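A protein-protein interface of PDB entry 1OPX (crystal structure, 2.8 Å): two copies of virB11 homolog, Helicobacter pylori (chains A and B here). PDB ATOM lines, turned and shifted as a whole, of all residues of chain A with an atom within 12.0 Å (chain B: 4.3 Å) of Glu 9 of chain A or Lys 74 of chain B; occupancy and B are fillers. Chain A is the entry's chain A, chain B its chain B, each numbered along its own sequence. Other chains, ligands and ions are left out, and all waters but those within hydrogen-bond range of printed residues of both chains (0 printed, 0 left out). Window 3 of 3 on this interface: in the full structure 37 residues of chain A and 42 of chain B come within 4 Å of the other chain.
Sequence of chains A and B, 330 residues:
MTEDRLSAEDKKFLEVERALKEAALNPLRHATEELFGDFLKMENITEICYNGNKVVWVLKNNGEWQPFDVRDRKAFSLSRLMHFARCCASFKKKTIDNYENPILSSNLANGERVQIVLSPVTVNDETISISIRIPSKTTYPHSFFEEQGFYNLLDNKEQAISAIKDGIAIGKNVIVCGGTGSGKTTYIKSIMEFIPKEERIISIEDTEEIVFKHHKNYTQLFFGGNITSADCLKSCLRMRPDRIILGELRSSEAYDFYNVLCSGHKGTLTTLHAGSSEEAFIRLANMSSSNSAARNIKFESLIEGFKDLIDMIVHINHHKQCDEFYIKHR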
ATOM      1  N   LEU A   6     -33.596 -27.381  -1.467  1.00  0.00           N
ATOM      2  CA  LEU A   6     -32.879 -27.767  -0.218  1.00  0.00           C
ATOM      3  C   LEU A   6     -31.483 -28.290  -0.575  1.00  0.00           C
ATOM      4  O   LEU A   6     -30.533 -28.120   0.190  1.00  0.00           O
ATOM      5  CB  LEU A   6     -33.687 -28.844   0.526  1.00  0.00           C
ATOM      6  CG  LEU A   6     -35.180 -28.504   0.699  1.00  0.00           C
ATOM      7  CD1 LEU A   6     -35.893 -29.668   1.399  1.00  0.00           C
ATOM      8  CD2 LEU A   6     -35.342 -27.188   1.489  1.00  0.00           C
ATOM      9  N   SER A   7     -31.375 -28.906  -1.751  1.00  0.00           N
ATOM     10  CA  SER A   7     -30.121 -29.468  -2.239  1.00  0.00           C
ATOM     11  C   SER A   7     -29.004 -28.449  -2.184  1.00  0.00           C
ATOM     12  O   SER A   7     -27.861 -28.799  -1.965  1.00  0.00           O
ATOM     13  CB  SER A   7     -30.284 -29.974  -3.674  1.00  0.00           C
ATOM     14  OG  SER A   7     -29.089 -30.566  -4.143  1.00  0.00           O
ATOM     15  N   ALA A   8     -29.337 -27.184  -2.377  1.00  0.00           N
ATOM     16  CA  ALA A   8     -28.327 -26.134  -2.336  1.00  0.00           C
ATOM     17  C   ALA A   8     -27.818 -25.918  -0.905  1.00  0.00           C
ATOM     18  O   ALA A   8     -26.612 -25.812  -0.666  1.00  0.00           O
ATOM     19  CB  ALA A   8     -28.908 -24.833  -2.896  1.00  0.00           C
ATOM     20  N   GLU A   9     -28.749 -25.857   0.043  1.00  0.00           N
ATOM     21  CA  GLU A   9     -28.406 -25.647   1.445  1.00  0.00           C
ATOM     22  C   GLU A   9     -27.755 -26.894   2.025  1.00  0.00           C
ATOM     23  O   GLU A   9     -26.862 -26.808   2.865  1.00  0.00           O
ATOM     24  CB  GLU A   9     -29.661 -25.289   2.261  1.00  0.00           C
ATOM     25  CG  GLU A   9     -30.293 -23.925   1.914  1.00  0.00           C
ATOM     26  CD  GLU A   9     -30.943 -23.883   0.525  1.00  0.00           C
ATOM     27  OE1 GLU A   9     -31.984 -24.548   0.336  1.00  0.00           O
ATOM     28  OE2 GLU A   9     -30.420 -23.190  -0.379  1.00  0.00           O
ATOM     29  N   ASP A  10     -28.210 -28.052   1.562  1.00  0.00           N
ATOM     30  CA  ASP A  10     -27.682 -29.317   2.038  1.00  0.00           C
ATOM     31  C   ASP A  10     -26.246 -29.543   1.572  1.00  0.00           C
ATOM     32  O   ASP A  10     -25.443 -30.129   2.302  1.00  0.00           O
ATOM     33  CB  ASP A  10     -28.588 -30.469   1.580  1.00  0.00           C
ATOM     34  CG  ASP A  10     -30.007 -30.364   2.153  1.00  0.00           C
ATOM     35  OD1 ASP A  10     -30.140 -29.919   3.316  1.00  0.00           O
ATOM     36  OD2 ASP A  10     -30.986 -30.737   1.454  1.00  0.00           O
ATOM     37  N   LYS A  11     -25.927 -29.059   0.372  1.00  0.00           N
ATOM     38  CA  LYS A  11     -24.587 -29.206  -0.212  1.00  0.00           C
ATOM     39  C   LYS A  11     -23.553 -28.465   0.622  1.00  0.00           C
ATOM     40  O   LYS A  11     -22.539 -29.037   1.021  1.00  0.00           O
ATOM     41  CB  LYS A  11     -24.569 -28.684  -1.661  1.00  0.00           C
ATOM     42  N   LYS A  12     -23.812 -27.192   0.890  1.00  0.00           N
ATOM     43  CA  LYS A  12     -22.894 -26.396   1.687  1.00  0.00           C
ATOM     44  C   LYS A  12     -22.704 -27.019   3.059  1.00  0.00           C
ATOM     45  O   LYS A  12     -21.612 -26.978   3.620  1.00  0.00           O
ATOM     46  CB  LYS A  12     -23.436 -24.975   1.813  1.00  0.00           C
ATOM     47  CG  LYS A  12     -23.687 -24.352   0.446  1.00  0.00           C
ATOM     48  CD  LYS A  12     -24.051 -22.872   0.482  1.00  0.00           C
ATOM     49  CE  LYS A  12     -24.137 -22.299  -0.945  1.00  0.00           C
ATOM     50  NZ  LYS A  12     -23.510 -20.928  -1.073  1.00  0.00           N
ATOM     51  N   PHE A  13     -23.779 -27.610   3.579  1.00  0.00           N
ATOM     52  CA  PHE A  13     -23.784 -28.265   4.891  1.00  0.00           C
ATOM     53  C   PHE A  13     -22.904 -29.501   4.916  1.00  0.00           C
ATOM     54  O   PHE A  13     -22.210 -29.748   5.891  1.00  0.00           O
ATOM     55  CB  PHE A  13     -25.205 -28.675   5.275  1.00  0.00           C
ATOM     56  CG  PHE A  13     -25.304 -29.392   6.598  1.00  0.00           C
ATOM     57  CD1 PHE A  13     -25.437 -28.682   7.794  1.00  0.00           C
ATOM     58  CD2 PHE A  13     -25.296 -30.780   6.646  1.00  0.00           C
ATOM     59  CE1 PHE A  13     -25.566 -29.350   9.013  1.00  0.00           C
ATOM     60  CE2 PHE A  13     -25.423 -31.454   7.855  1.00  0.00           C
ATOM     61  CZ  PHE A  13     -25.559 -30.742   9.036  1.00  0.00           C
ATOM     62  N   LEU A  14     -22.948 -30.288   3.847  1.00  0.00           N
ATOM     63  CA  LEU A  14     -22.141 -31.501   3.768  1.00  0.00           C
ATOM     64  C   LEU A  14     -20.703 -31.215   3.338  1.00  0.00           C
ATOM     65  O   LEU A  14     -19.771 -31.941   3.695  1.00  0.00           O
ATOM     66  CB  LEU A  14     -22.761 -32.489   2.783  1.00  0.00           C
ATOM     67  CG  LEU A  14     -24.065 -33.161   3.179  1.00  0.00           C
ATOM     68  CD1 LEU A  14     -24.315 -34.251   2.178  1.00  0.00           C
ATOM     69  CD2 LEU A  14     -23.989 -33.745   4.582  1.00  0.00           C
ATOM     70  N   GLU A  15     -20.543 -30.152   2.563  1.00  0.00           N
ATOM     71  CA  GLU A  15     -19.255 -29.740   2.040  1.00  0.00           C
ATOM     72  C   GLU A  15     -18.026 -30.095   2.854  1.00  0.00           C
ATOM     73  O   GLU A  15     -17.050 -30.587   2.300  1.00  0.00           O
ATOM     74  CB  GLU A  15     -19.257 -28.242   1.812  1.00  0.00           C
ATOM     75  CG  GLU A  15     -18.033 -27.770   1.119  1.00  0.00           C
ATOM     76  CD  GLU A  15     -17.939 -26.292   1.164  1.00  0.00           C
ATOM     77  OE1 GLU A  15     -18.107 -25.747   2.281  1.00  0.00           O
ATOM     78  OE2 GLU A  15     -17.696 -25.690   0.096  1.00  0.00           O
ATOM     79  N   VAL A  16     -18.065 -29.846   4.158  1.00  0.00           N
ATOM     80  CA  VAL A  16     -16.910 -30.116   5.017  1.00  0.00           C
ATOM     81  C   VAL A  16     -16.588 -31.578   5.348  1.00  0.00           C
ATOM     82  O   VAL A  16     -15.411 -31.951   5.489  1.00  0.00           O
ATOM     83  CB  VAL A  16     -17.031 -29.321   6.319  1.00  0.00           C
ATOM     84  CG1 VAL A  16     -15.828 -29.605   7.238  1.00  0.00           C
ATOM     85  CG2 VAL A  16     -17.134 -27.831   5.977  1.00  0.00           C
ATOM     86  N   GLU A  17     -17.615 -32.408   5.494  1.00  0.00           N
ATOM     87  CA  GLU A  17     -17.377 -33.821   5.774  1.00  0.00           C
ATOM     88  C   GLU A  17     -16.967 -34.523   4.484  1.00  0.00           C
ATOM     89  O   GLU A  17     -16.049 -35.344   4.483  1.00  0.00           O
ATOM     90  CB  GLU A  17     -18.626 -34.489   6.348  1.00  0.00           C
ATOM     91  CG  GLU A  17     -18.763 -34.350   7.857  1.00  0.00           C
ATOM     92  CD  GLU A  17     -17.601 -34.969   8.612  1.00  0.00           C
ATOM     93  OE1 GLU A  17     -17.368 -36.189   8.445  1.00  0.00           O
ATOM     94  OE2 GLU A  17     -16.921 -34.236   9.370  1.00  0.00           O
ATOM     95  N   ARG A  18     -17.638 -34.186   3.386  1.00  0.00           N
ATOM     96  CA  ARG A  18     -17.325 -34.794   2.104  1.00  0.00           C
ATOM     97  C   ARG A  18     -15.881 -34.559   1.710  1.00  0.00           C
ATOM     98  O   ARG A  18     -15.204 -35.485   1.283  1.00  0.00           O
ATOM     99  CB  ARG A  18     -18.269 -34.275   1.021  1.00  0.00           C
ATOM    100  CG  ARG A  18     -19.693 -34.804   1.176  1.00  0.00           C
ATOM    101  CD  ARG A  18     -20.525 -34.560  -0.053  1.00  0.00           C
ATOM    102  NE  ARG A  18     -21.843 -35.179   0.043  1.00  0.00           N
ATOM    103  CZ  ARG A  18     -22.766 -35.083  -0.909  1.00  0.00           C
ATOM    104  NH1 ARG A  18     -22.494 -34.393  -2.014  1.00  0.00           N
ATOM    105  NH2 ARG A  18     -23.952 -35.668  -0.764  1.00  0.00           N
ATOM    106  N   ARG B  73     -40.108 -28.930   2.169  1.00  0.00           N
ATOM    107  CA  ARG B  73     -40.167 -28.241   3.457  1.00  0.00           C
ATOM    108  C   ARG B  73     -38.747 -27.910   3.917  1.00  0.00           C
ATOM    109  O   ARG B  73     -37.848 -28.758   3.839  1.00  0.00           O
ATOM    110  CB  ARG B  73     -40.876 -29.093   4.511  1.00  0.00           C
ATOM    111  CG  ARG B  73     -42.350 -29.321   4.247  1.00  0.00           C
ATOM    112  CD  ARG B  73     -43.038 -29.933   5.469  1.00  0.00           C
ATOM    113  NE  ARG B  73     -44.487 -30.052   5.291  1.00  0.00           N
ATOM    114  CZ  ARG B  73     -45.349 -30.410   6.245  1.00  0.00           C
ATOM    115  NH1 ARG B  73     -44.927 -30.693   7.470  1.00  0.00           N
ATOM    116  NH2 ARG B  73     -46.645 -30.467   5.980  1.00  0.00           N
ATOM    117  N   LYS B  74     -38.542 -26.672   4.365  1.00  0.00           N
ATOM    118  CA  LYS B  74     -37.231 -26.249   4.821  1.00  0.00           C
ATOM    119  C   LYS B  74     -36.843 -27.136   6.007  1.00  0.00           C
ATOM    120  O   LYS B  74     -35.709 -27.609   6.087  1.00  0.00           O
ATOM    121  CB  LYS B  74     -37.264 -24.762   5.221  1.00  0.00           C
ATOM    122  CG  LYS B  74     -35.941 -24.178   5.775  1.00  0.00           C
ATOM    123  CD  LYS B  74     -34.801 -24.195   4.755  1.00  0.00           C
ATOM    124  CE  LYS B  74     -33.488 -23.704   5.371  1.00  0.00           C
ATOM    125  NZ  LYS B  74     -32.303 -23.995   4.496  1.00  0.00           N
ATOM    126  N   ALA B  75     -37.800 -27.382   6.901  1.00  0.00           N
ATOM    127  CA  ALA B  75     -37.585 -28.202   8.090  1.00  0.00           C
ATOM    128  C   ALA B  75     -36.841 -29.504   7.828  1.00  0.00           C
ATOM    129  O   ALA B  75     -36.092 -29.978   8.681  1.00  0.00           O
ATOM    130  CB  ALA B  75     -38.916 -28.507   8.756  1.00  0.00           C
ATOM    131  N   PHE B  76     -37.040 -30.097   6.659  1.00  0.00           N
ATOM    132  CA  PHE B  76     -36.368 -31.346   6.371  1.00  0.00           C
ATOM    133  C   PHE B  76     -35.140 -31.214   5.478  1.00  0.00           C
ATOM    134  O   PHE B  76     -35.041 -31.829   4.413  1.00  0.00           O
ATOM    135  CB  PHE B  76     -37.371 -32.357   5.808  1.00  0.00           C
ATOM    136  CG  PHE B  76     -38.366 -32.851   6.833  1.00  0.00           C
ATOM    137  CD1 PHE B  76     -39.510 -32.108   7.136  1.00  0.00           C
ATOM    138  CD2 PHE B  76     -38.137 -34.044   7.524  1.00  0.00           C
ATOM    139  CE1 PHE B  76     -40.411 -32.545   8.112  1.00  0.00           C
ATOM    140  CE2 PHE B  76     -39.019 -34.490   8.495  1.00  0.00           C
ATOM    141  CZ  PHE B  76     -40.163 -33.740   8.793  1.00  0.00           C
ATOM    142  N   SER B  77     -34.204 -30.396   5.954  1.00  0.00           N
ATOM    143  CA  SER B  77     -32.919 -30.136   5.303  1.00  0.00           C
ATOM    144  C   SER B  77     -31.838 -30.565   6.287  1.00  0.00           C
ATOM    145  O   SER B  77     -31.940 -30.303   7.492  1.00  0.00           O
ATOM    146  CB  SER B  77     -32.742 -28.655   4.999  1.00  0.00           C
ATOM    147  OG  SER B  77     -33.601 -28.274   3.955  1.00  0.00           O
ATOM    148  N   ARG B  80     -31.362 -28.367   8.957  1.00  0.00           N
ATOM    149  CA  ARG B  80     -32.546 -28.290   9.817  1.00  0.00           C
ATOM    150  C   ARG B  80     -32.728 -29.544  10.655  1.00  0.00           C
ATOM    151  O   ARG B  80     -33.115 -29.473  11.824  1.00  0.00           O
ATOM    152  CB  ARG B  80     -33.799 -28.060   8.972  1.00  0.00           C
ATOM    153  CG  ARG B  80     -34.002 -26.631   8.462  1.00  0.00           C
ATOM    154  CD  ARG B  80     -34.295 -25.668   9.587  1.00  0.00           C
ATOM    155  NE  ARG B  80     -33.068 -25.064  10.096  1.00  0.00           N
ATOM    156  CZ  ARG B  80     -32.936 -24.468  11.286  1.00  0.00           C
ATOM    157  NH1 ARG B  80     -33.970 -24.395  12.124  1.00  0.00           N
ATOM    158  NH2 ARG B  80     -31.765 -23.933  11.636  1.00  0.00           N
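The side-chain hydroxyl (OG) of Ser 77 of chain B sits at hydrogen-bond distance from the backbone carbonyl oxygen (O) of Lys 74 of chain B, at 3.1 Å.
CD1 of Leu 6 of chain A touches O of Arg 73 of chain B, at 3.3 Å. Lys 74 of chain B touches Leu 6 of chain A. Phe 76 of chain B touches Leu 6 of chain A. Leu 6 of chain A touches Ser 77 of chain B (CD2 to OG, 3.2 Å). Glu 9 of chain A touches Lys 74 of chain B. Ser 77 of chain B touches Asp 10 of chain A.
Of the printed residues of chain B, Leu 6 of chain A touches Arg 73, Lys 74, Phe 76 and Ser 77. Glu 9 of chain A touches just one residue of chain B: Lys 74 (3.3 Å). Of the printed residues of chain B, Asp 10 of chain A touches Ser 77. Of the printed residues of chain A, Arg 73 of chain B touches Leu 6. Of the printed residues of chain A, Lys 74 of chain B touches Leu 6 and Glu 9. Ala 75 of chain B touches none of the printed residues of chain A. Of the printed residues of chain A, Phe 76 of chain B touches Leu 6 (3.8 Å). Ser 77 of chain B touches two residues of chain A. The nearest residue of chain A that does not touch Lys 74 of chain B is Asp 10 of chain A (6.4 Å). The nearest printed residue of chain A that does not touch Arg 73 of chain B is Asp 10 of chain A (7.5 Å).
Of the 13 printed residues of chain A, 3 touch a printed residue of chain B. Printed residues of chain A that touch a printed residue of chain B: Leu 6, Glu 9 and Asp 10. Hydrophobic or aromatic side chains of chain A that line the printed part of chain B: Leu 6. Among the printed residues, 6 pairs touch across the chains. Among the printed residues, no Asp or Glu carboxylate lies within 4 Å of a Lys or Arg side-chain nitrogen of the other chain.
No position is printed for both chains. Of the 6 pairs that touch across the chains among the printed residues, none has its exchanged pair printed and touching as well.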
